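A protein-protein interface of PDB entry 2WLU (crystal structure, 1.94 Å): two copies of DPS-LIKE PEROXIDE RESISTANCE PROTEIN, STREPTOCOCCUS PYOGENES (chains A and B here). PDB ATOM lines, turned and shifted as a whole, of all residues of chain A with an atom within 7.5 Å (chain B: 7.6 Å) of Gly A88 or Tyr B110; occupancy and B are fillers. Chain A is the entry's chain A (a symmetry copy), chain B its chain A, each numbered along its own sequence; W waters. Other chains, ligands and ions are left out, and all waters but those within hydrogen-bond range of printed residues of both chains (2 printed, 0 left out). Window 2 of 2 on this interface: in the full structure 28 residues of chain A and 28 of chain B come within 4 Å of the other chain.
The side-chain hydroxyl (OH) of Tyr B52 is in hydrogen-bond range of the backbone carbonyl oxygen (O) of Pro A90, at 2.5 Å.
The side-chain hydroxyl (OH) of Tyr B110 is in hydrogen-bond range of the backbone carbonyl oxygen (O) of Gly A88, at 2.7 Å.
The backbone carbonyl oxygen of Glu A81 lies within hydrogen-bond range of the side-chain hydroxyl of Thr A85 (2.7 Å).
O of Ala A89 sits close to OD1 of Asn A33.
The backbone carbonyl oxygen of Leu A83 sits at hydrogen-bond distance from the backbone NH of Gly A88, at 2.7 Å.
Ser A80 touches Trp B51.
Glu A81 touches Trp B51.
Trp B51 touches Ile A84 (O to CD1, 3.5 Å).
Tyr B110 touches Ile A84 (OH to CG2, 3.5 Å).
Ala A89 touches Tyr B52.
Ala A89 touches Tyr B110 (CA to OH, 3.7 Å).
OH of Tyr B110 touches CD of Pro A90 (3.6 Å).
Tyr B110 touches four residues of chain A.
No residue of chain B comes within 4 Å of Gly A87.
Printed residues of chain A within 4 Å of Tyr B52: Ala A89 and Pro A90.
Printed residues of chain B within 4 Å of Ser A80: Trp B51.
Of the printed residues of chain B, Ala A89 touches Tyr B52 and Tyr B110.
Asn A25 touches none of the printed residues of chain B.
Thr A85 touches none of the printed residues of chain B.
The nearest residue of chain B that does not touch Gly A88 is Tyr B52 (5.7 Å).
Of the 14 printed residues of chain A, 6 touch a printed residue of chain B.
Printed residues of chain A that touch a printed residue of chain B: Ser A80, Glu A81, Ile A84, Gly A88, Ala A89 and Pro A90.
Hydrophobic or aromatic side chains of chain B that line the printed part of chain A: Trp B51, Tyr B52 and Tyr B110.
No position is printed for both chains.
Of the 9 pairs that touch across the chains among the printed residues, none has its exchanged pair printed and touching as well.
Water W2 lies within hydrogen-bond range of the backbone carbonyl oxygen of Ile A84 (2.7 Å), the backbone carbonyl oxygen of Gly A88 (2.9 Å) and the side-chain hydroxyl of Tyr B110 (3.4 Å).
Water W1 lies within hydrogen-bond range of N of Gly B108 and O of Pro A90.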
ATOM      1  N   ASN A  25      17.589 -19.285  24.733  1.00  0.00           N
ATOM      2  CA  ASN A  25      16.248 -19.684  25.175  1.00  0.00           C
ATOM      3  C   ASN A  25      15.469 -20.551  24.176  1.00  0.00           C
ATOM      4  O   ASN A  25      14.237 -20.495  24.120  1.00  0.00           O
ATOM      5  CB  ASN A  25      15.421 -18.467  25.638  1.00  0.00           C
ATOM      6  CG  ASN A  25      15.082 -17.496  24.501  1.00  0.00           C
ATOM      7  OD1 ASN A  25      15.593 -17.608  23.385  1.00  0.00           O
ATOM      8  ND2 ASN A  25      14.209 -16.536  24.792  1.00  0.00           N
ATOM      9  N   LYS A  29      11.403 -21.432  24.080  1.00  0.00           N
ATOM     10  CA  LYS A  29      10.575 -21.071  22.928  1.00  0.00           C
ATOM     11  C   LYS A  29       9.841 -22.294  22.374  1.00  0.00           C
ATOM     12  O   LYS A  29       8.663 -22.205  22.012  1.00  0.00           O
ATOM     13  CB  LYS A  29      11.401 -20.373  21.835  1.00  0.00           C
ATOM     14  CG  LYS A  29      11.888 -18.987  22.246  1.00  0.00           C
ATOM     15  CD  LYS A  29      12.480 -18.204  21.074  1.00  0.00           C
ATOM     16  CE  LYS A  29      13.838 -18.728  20.669  1.00  0.00           C
ATOM     17  NZ  LYS A  29      14.428 -17.898  19.551  1.00  0.00           N
ATOM     18  N   ASN A  33       5.754 -22.902  22.242  1.00  0.00           N
ATOM     19  CA  ASN A  33       5.072 -23.143  20.970  1.00  0.00           C
ATOM     20  C   ASN A  33       4.268 -24.449  20.992  1.00  0.00           C
ATOM     21  O   ASN A  33       3.169 -24.515  20.439  1.00  0.00           O
ATOM     22  CB  ASN A  33       6.053 -23.107  19.784  1.00  0.00           C
ATOM     23  CG  ASN A  33       5.447 -22.455  18.537  1.00  0.00           C
ATOM     24  OD1 ASN A  33       6.022 -22.520  17.439  1.00  0.00           O
ATOM     25  ND2 ASN A  33       4.295 -21.832  18.697  1.00  0.00           N
ATOM     26  N   SER A  80       1.141 -17.428  23.874  1.00  0.00           N
ATOM     27  CA  SER A  80       1.568 -16.968  22.556  1.00  0.00           C
ATOM     28  C   SER A  80       2.306 -15.634  22.664  1.00  0.00           C
ATOM     29  O   SER A  80       3.387 -15.458  22.089  1.00  0.00           O
ATOM     30  CB  SER A  80       0.363 -16.854  21.614  1.00  0.00           C
ATOM     31  OG  SER A  80       0.750 -16.364  20.345  1.00  0.00           O
ATOM     32  N   GLU A  81       1.728 -14.695  23.411  1.00  0.00           N
ATOM     33  CA  GLU A  81       2.360 -13.379  23.553  1.00  0.00           C
ATOM     34  C   GLU A  81       3.670 -13.422  24.341  1.00  0.00           C
ATOM     35  O   GLU A  81       4.576 -12.626  24.080  1.00  0.00           O
ATOM     36  CB  GLU A  81       1.369 -12.347  24.091  1.00  0.00           C
ATOM     37  CG  GLU A  81       0.252 -12.121  23.062  1.00  0.00           C
ATOM     38  CD  GLU A  81      -0.865 -11.227  23.543  1.00  0.00           C
ATOM     39  OE1 GLU A  81      -0.821 -10.738  24.698  1.00  0.00           O
ATOM     40  OE2 GLU A  81      -1.796 -11.012  22.738  1.00  0.00           O
ATOM     41  N   ARG A  82       3.787 -14.355  25.283  1.00  0.00           N
ATOM     42  CA  ARG A  82       5.070 -14.541  25.982  1.00  0.00           C
ATOM     43  C   ARG A  82       6.128 -15.045  25.000  1.00  0.00           C
ATOM     44  O   ARG A  82       7.286 -14.605  25.030  1.00  0.00           O
ATOM     45  CB  ARG A  82       4.920 -15.504  27.171  1.00  0.00           C
ATOM     46  CG  ARG A  82       6.203 -15.727  27.990  1.00  0.00           C
ATOM     47  CD  ARG A  82       6.641 -14.448  28.715  1.00  0.00           C
ATOM     48  NE  ARG A  82       7.921 -14.637  29.404  1.00  0.00           N
ATOM     49  CZ  ARG A  82       8.699 -13.651  29.839  1.00  0.00           C
ATOM     50  NH1 ARG A  82       8.336 -12.380  29.681  1.00  0.00           N
ATOM     51  NH2 ARG A  82       9.849 -13.942  30.444  1.00  0.00           N
ATOM     52  N   LEU A  83       5.722 -15.951  24.116  1.00  0.00           N
ATOM     53  CA  LEU A  83       6.612 -16.473  23.083  1.00  0.00           C
ATOM     54  C   LEU A  83       7.087 -15.370  22.122  1.00  0.00           C
ATOM     55  O   LEU A  83       8.283 -15.294  21.800  1.00  0.00           O
ATOM     56  CB  LEU A  83       5.948 -17.640  22.331  1.00  0.00           C
ATOM     57  CG  LEU A  83       6.738 -18.240  21.149  1.00  0.00           C
ATOM     58  CD1 LEU A  83       8.129 -18.711  21.578  1.00  0.00           C
ATOM     59  CD2 LEU A  83       5.956 -19.380  20.511  1.00  0.00           C
ATOM     60  N   ILE A  84       6.165 -14.519  21.675  1.00  0.00           N
ATOM     61  CA  ILE A  84       6.513 -13.346  20.856  1.00  0.00           C
ATOM     62  C   ILE A  84       7.517 -12.462  21.605  1.00  0.00           C
ATOM     63  O   ILE A  84       8.569 -12.084  21.066  1.00  0.00           O
ATOM     64  CB  ILE A  84       5.267 -12.476  20.534  1.00  0.00           C
ATOM     65  CG1 ILE A  84       4.188 -13.280  19.790  1.00  0.00           C
ATOM     66  CG2 ILE A  84       5.664 -11.238  19.696  1.00  0.00           C
ATOM     67  CD1 ILE A  84       2.842 -12.564  19.737  1.00  0.00           C
ATOM     68  N   THR A  85       7.177 -12.159  22.854  1.00  0.00           N
ATOM     69  CA  THR A  85       7.947 -11.271  23.723  1.00  0.00           C
ATOM     70  C   THR A  85       9.408 -11.711  23.895  1.00  0.00           C
ATOM     71  O   THR A  85      10.326 -10.873  23.837  1.00  0.00           O
ATOM     72  CB  THR A  85       7.217 -11.114  25.074  1.00  0.00           C
ATOM     73  OG1 THR A  85       5.965 -10.459  24.838  1.00  0.00           O
ATOM     74  CG2 THR A  85       8.030 -10.299  26.072  1.00  0.00           C
ATOM     75  N   ILE A  86       9.625 -13.018  24.055  1.00  0.00           N
ATOM     76  CA  ILE A  86      10.982 -13.546  24.248  1.00  0.00           C
ATOM     77  C   ILE A  86      11.716 -13.853  22.931  1.00  0.00           C
ATOM     78  O   ILE A  86      12.786 -14.466  22.943  1.00  0.00           O
ATOM     79  CB  ILE A  86      11.021 -14.740  25.257  1.00  0.00           C
ATOM     80  CG1 ILE A  86      10.382 -16.002  24.661  1.00  0.00           C
ATOM     81  CG2 ILE A  86      10.343 -14.332  26.602  1.00  0.00           C
ATOM     82  CD1 ILE A  86      10.682 -17.275  25.456  1.00  0.00           C
ATOM     83  N   GLY A  87      11.127 -13.444  21.807  1.00  0.00           N
ATOM     84  CA  GLY A  87      11.794 -13.518  20.503  1.00  0.00           C
ATOM     85  C   GLY A  87      11.403 -14.684  19.613  1.00  0.00           C
ATOM     86  O   GLY A  87      12.091 -14.975  18.640  1.00  0.00           O
ATOM     87  N   GLY A  88      10.296 -15.351  19.938  1.00  0.00           N
ATOM     88  CA  GLY A  88       9.809 -16.480  19.142  1.00  0.00           C
ATOM     89  C   GLY A  88       8.702 -16.141  18.158  1.00  0.00           C
ATOM     90  O   GLY A  88       8.373 -14.974  17.940  1.00  0.00           O
ATOM     91  N   ALA A  89       8.119 -17.176  17.565  1.00  0.00           N
ATOM     92  CA  ALA A  89       7.099 -17.006  16.534  1.00  0.00           C
ATOM     93  C   ALA A  89       6.035 -18.075  16.728  1.00  0.00           C
ATOM     94  O   ALA A  89       6.263 -19.236  16.401  1.00  0.00           O
ATOM     95  CB  ALA A  89       7.734 -17.098  15.135  1.00  0.00           C
ATOM     96  N   PRO A  90       4.873 -17.696  17.286  1.00  0.00           N
ATOM     97  CA  PRO A  90       3.870 -18.711  17.614  1.00  0.00           C
ATOM     98  C   PRO A  90       3.147 -19.289  16.404  1.00  0.00           C
ATOM     99  O   PRO A  90       2.921 -18.576  15.410  1.00  0.00           O
ATOM    100  CB  PRO A  90       2.876 -17.947  18.494  1.00  0.00           C
ATOM    101  CG  PRO A  90       2.994 -16.505  18.016  1.00  0.00           C
ATOM    102  CD  PRO A  90       4.482 -16.354  17.766  1.00  0.00           C
ATOM    103  N   GLN B  48      -3.983 -14.322  14.156  1.00  0.00           N
ATOM    104  CA  GLN B  48      -2.649 -14.157  13.569  1.00  0.00           C
ATOM    105  C   GLN B  48      -2.293 -12.674  13.415  1.00  0.00           C
ATOM    106  O   GLN B  48      -1.154 -12.277  13.673  1.00  0.00           O
ATOM    107  CB  GLN B  48      -2.566 -14.857  12.213  1.00  0.00           C
ATOM    108  CG  GLN B  48      -1.175 -14.794  11.566  1.00  0.00           C
ATOM    109  CD  GLN B  48      -1.147 -15.557  10.266  1.00  0.00           C
ATOM    110  OE1 GLN B  48      -1.536 -15.037   9.224  1.00  0.00           O
ATOM    111  NE2 GLN B  48      -0.727 -16.810  10.329  1.00  0.00           N
ATOM    112  N   TRP B  51      -1.405 -11.157  16.794  1.00  0.00           N
ATOM    113  CA  TRP B  51      -0.087 -11.520  17.315  1.00  0.00           C
ATOM    114  C   TRP B  51       1.091 -10.987  16.495  1.00  0.00           C
ATOM    115  O   TRP B  51       2.073 -10.514  17.066  1.00  0.00           O
ATOM    116  CB  TRP B  51       0.029 -13.042  17.471  1.00  0.00           C
ATOM    117  CG  TRP B  51      -0.842 -13.611  18.572  1.00  0.00           C
ATOM    118  CD1 TRP B  51      -1.228 -12.993  19.731  1.00  0.00           C
ATOM    119  CD2 TRP B  51      -1.411 -14.925  18.606  1.00  0.00           C
ATOM    120  NE1 TRP B  51      -2.016 -13.848  20.487  1.00  0.00           N
ATOM    121  CE2 TRP B  51      -2.145 -15.035  19.814  1.00  0.00           C
ATOM    122  CE3 TRP B  51      -1.371 -16.021  17.732  1.00  0.00           C
ATOM    123  CZ2 TRP B  51      -2.833 -16.206  20.174  1.00  0.00           C
ATOM    124  CZ3 TRP B  51      -2.062 -17.190  18.086  1.00  0.00           C
ATOM    125  CH2 TRP B  51      -2.781 -17.267  19.306  1.00  0.00           C
ATOM    126  N   TYR B  52       0.986 -11.070  15.169  1.00  0.00           N
ATOM    127  CA  TYR B  52       2.124 -10.805  14.272  1.00  0.00           C
ATOM    128  C   TYR B  52       2.300  -9.356  13.793  1.00  0.00           C
ATOM    129  O   TYR B  52       3.368  -8.995  13.283  1.00  0.00           O
ATOM    130  CB  TYR B  52       2.085 -11.758  13.065  1.00  0.00           C
ATOM    131  CG  TYR B  52       2.678 -13.113  13.380  1.00  0.00           C
ATOM    132  CD1 TYR B  52       4.041 -13.363  13.172  1.00  0.00           C
ATOM    133  CD2 TYR B  52       1.890 -14.137  13.906  1.00  0.00           C
ATOM    134  CE1 TYR B  52       4.605 -14.603  13.477  1.00  0.00           C
ATOM    135  CE2 TYR B  52       2.441 -15.378  14.221  1.00  0.00           C
ATOM    136  CZ  TYR B  52       3.796 -15.600  14.002  1.00  0.00           C
ATOM    137  OH  TYR B  52       4.351 -16.819  14.294  1.00  0.00           O
ATOM    138  N   MET B  53       1.269  -8.527  13.960  1.00  0.00           N
ATOM    139  CA  MET B  53       1.327  -7.139  13.482  1.00  0.00           C
ATOM    140  C   MET B  53       2.493  -6.321  14.073  1.00  0.00           C
ATOM    141  O   MET B  53       2.776  -6.384  15.279  1.00  0.00           O
ATOM    142  CB  MET B  53      -0.003  -6.413  13.738  1.00  0.00           C
ATOM    143  CG  MET B  53      -0.008  -4.943  13.262  1.00  0.00           C
ATOM    144  SD  MET B  53      -1.580  -4.097  13.579  1.00  0.00           S
ATOM    145  CE  MET B  53      -2.549  -4.695  12.198  1.00  0.00           C
ATOM    146  N   ARG B  54       3.162  -5.562  13.203  1.00  0.00           N
ATOM    147  CA  ARG B  54       4.118  -4.535  13.615  1.00  0.00           C
ATOM    148  C   ARG B  54       3.882  -3.308  12.756  1.00  0.00           C
ATOM    149  O   ARG B  54       3.654  -3.426  11.544  1.00  0.00           O
ATOM    150  CB  ARG B  54       5.570  -4.987  13.405  1.00  0.00           C
ATOM    151  CG  ARG B  54       6.038  -6.172  14.238  1.00  0.00           C
ATOM    152  CD  ARG B  54       7.510  -6.440  13.919  1.00  0.00           C
ATOM    153  NE  ARG B  54       8.048  -7.600  14.618  1.00  0.00           N
ATOM    154  CZ  ARG B  54       9.214  -8.172  14.311  1.00  0.00           C
ATOM    155  NH1 ARG B  54       9.958  -7.696  13.321  1.00  0.00           N
ATOM    156  NH2 ARG B  54       9.627  -9.225  14.981  1.00  0.00           N
ATOM    157  N   GLY B  55       3.947  -2.133  13.372  1.00  0.00           N
ATOM    158  CA  GLY B  55       3.832  -0.888  12.629  1.00  0.00           C
ATOM    159  C   GLY B  55       2.984   0.131  13.352  1.00  0.00           C
ATOM    160  O   GLY B  55       2.247  -0.220  14.288  1.00  0.00           O
ATOM    161  N   LYS B 107       1.412 -19.402   7.054  1.00  0.00           N
ATOM    162  CA  LYS B 107       2.309 -19.301   8.203  1.00  0.00           C
ATOM    163  C   LYS B 107       2.467 -17.827   8.600  1.00  0.00           C
ATOM    164  O   LYS B 107       2.641 -16.954   7.736  1.00  0.00           O
ATOM    165  CB  LYS B 107       3.670 -19.910   7.847  1.00  0.00           C
ATOM    166  CG  LYS B 107       4.618 -20.152   9.021  1.00  0.00           C
ATOM    167  CD  LYS B 107       6.013 -20.552   8.500  1.00  0.00           C
ATOM    168  CE  LYS B 107       6.940 -21.017   9.619  1.00  0.00           C
ATOM    169  NZ  LYS B 107       7.181 -19.958  10.648  1.00  0.00           N
ATOM    170  N   GLY B 108       2.388 -17.551   9.896  1.00  0.00           N
ATOM    171  CA  GLY B 108       2.607 -16.192  10.390  1.00  0.00           C
ATOM    172  C   GLY B 108       4.018 -15.704  10.102  1.00  0.00           C
ATOM    173  O   GLY B 108       4.977 -16.481  10.168  1.00  0.00           O
ATOM    174  N   THR B 109       4.124 -14.428   9.732  1.00  0.00           N
ATOM    175  CA  THR B 109       5.413 -13.767   9.590  1.00  0.00           C
ATOM    176  C   THR B 109       5.317 -12.319  10.062  1.00  0.00           C
ATOM    177  O   THR B 109       4.321 -11.626   9.801  1.00  0.00           O
ATOM    178  CB  THR B 109       5.973 -13.847   8.139  1.00  0.00           C
ATOM    179  OG1 THR B 109       7.116 -12.994   8.023  1.00  0.00           O
ATOM    180  CG2 THR B 109       4.928 -13.425   7.105  1.00  0.00           C
ATOM    181  N   TYR B 110       6.344 -11.873  10.785  1.00  0.00           N
ATOM    182  CA  TYR B 110       6.364 -10.498  11.305  1.00  0.00           C
ATOM    183  C   TYR B 110       6.592  -9.446  10.222  1.00  0.00           C
ATOM    184  O   TYR B 110       6.400  -8.256  10.467  1.00  0.00           O
ATOM    185  CB  TYR B 110       7.412 -10.326  12.406  1.00  0.00           C
ATOM    186  CG  TYR B 110       7.131 -11.147  13.647  1.00  0.00           C
ATOM    187  CD1 TYR B 110       6.071 -10.811  14.507  1.00  0.00           C
ATOM    188  CD2 TYR B 110       7.924 -12.246  13.967  1.00  0.00           C
ATOM    189  CE1 TYR B 110       5.812 -11.558  15.649  1.00  0.00           C
ATOM    190  CE2 TYR B 110       7.669 -13.011  15.116  1.00  0.00           C
ATOM    191  CZ  TYR B 110       6.610 -12.658  15.945  1.00  0.00           C
ATOM    192  OH  TYR B 110       6.354 -13.403  17.078  1.00  0.00           O
ATOM    193  N   ASP B 111       6.985  -9.875   9.026  1.00  0.00           N
ATOM    194  CA  ASP B 111       7.317  -8.891   7.990  1.00  0.00           C
ATOM    195  C   ASP B 111       6.123  -8.427   7.146  1.00  0.00           C
ATOM    196  O   ASP B 111       6.283  -7.574   6.274  1.00  0.00           O
ATOM    197  CB  ASP B 111       8.512  -9.339   7.132  1.00  0.00           C
ATOM    198  CG  ASP B 111       8.215 -10.544   6.266  1.00  0.00           C
ATOM    199  OD1 ASP B 111       7.057 -11.007   6.202  1.00  0.00           O
ATOM    200  OD2 ASP B 111       9.165 -11.042   5.630  1.00  0.00           O
ATOM    201  N   LYS B 112       4.941  -8.981   7.414  1.00  0.00           N
ATOM    202  CA  LYS B 112       3.701  -8.478   6.815  1.00  0.00           C
ATOM    203  C   LYS B 112       3.454  -7.057   7.295  1.00  0.00           C
ATOM    204  O   LYS B 112       3.640  -6.756   8.479  1.00  0.00           O
ATOM    205  CB  LYS B 112       2.503  -9.353   7.200  1.00  0.00           C
ATOM    206  CG  LYS B 112       2.461 -10.728   6.553  1.00  0.00           C
ATOM    207  CD  LYS B 112       1.843 -10.697   5.161  1.00  0.00           C
ATOM    208  CE  LYS B 112       1.778 -12.098   4.570  1.00  0.00           C
ATOM    209  NZ  LYS B 112       1.711 -12.062   3.080  1.00  0.00           N
ATOM    210  N   THR B 113       3.047  -6.169   6.385  1.00  0.00           N
ATOM    211  CA  THR B 113       2.794  -4.769   6.759  1.00  0.00           C
ATOM    212  C   THR B 113       1.387  -4.625   7.340  1.00  0.00           C
ATOM    213  O   THR B 113       0.554  -5.521   7.175  1.00  0.00           O
ATOM    214  CB  THR B 113       2.936  -3.790   5.567  1.00  0.00           C
ATOM    215  OG1 THR B 113       1.902  -4.054   4.609  1.00  0.00           O
ATOM    216  CG2 THR B 113       4.324  -3.914   4.893  1.00  0.00           C
ATOM    217  N   VAL B 114       1.132  -3.502   8.012  1.00  0.00           N
ATOM    218  CA  VAL B 114      -0.208  -3.178   8.521  1.00  0.00           C
ATOM    219  C   VAL B 114      -1.217  -3.175   7.368  1.00  0.00           C
ATOM    220  O   VAL B 114      -2.294  -3.767   7.481  1.00  0.00           O
ATOM    221  CB  VAL B 114      -0.227  -1.827   9.290  1.00  0.00           C
ATOM    222  CG1 VAL B 114      -1.671  -1.311   9.504  1.00  0.00           C
ATOM    223  CG2 VAL B 114       0.504  -1.961  10.637  1.00  0.00           C
ATOM    224  N   HIS B 117      -2.182  -6.720   6.395  1.00  0.00           N
ATOM    225  CA  HIS B 117      -3.113  -7.304   7.372  1.00  0.00           C
ATOM    226  C   HIS B 117      -4.532  -6.774   7.147  1.00  0.00           C
ATOM    227  O   HIS B 117      -5.485  -7.547   7.121  1.00  0.00           O
ATOM    228  CB  HIS B 117      -2.657  -7.026   8.820  1.00  0.00           C
ATOM    229  CG  HIS B 117      -1.455  -7.817   9.253  1.00  0.00           C
ATOM    230  ND1 HIS B 117      -1.400  -9.194   9.192  1.00  0.00           N
ATOM    231  CD2 HIS B 117      -0.269  -7.421   9.780  1.00  0.00           C
ATOM    232  CE1 HIS B 117      -0.234  -9.611   9.657  1.00  0.00           C
ATOM    233  NE2 HIS B 117       0.469  -8.554  10.025  1.00  0.00           N
HETATM  234  O   HOH W   1       2.272 -19.389  12.164  1.00  0.00           O
HETATM  235  O   HOH W   2       9.304 -12.324  18.436  1.00  0.00           O
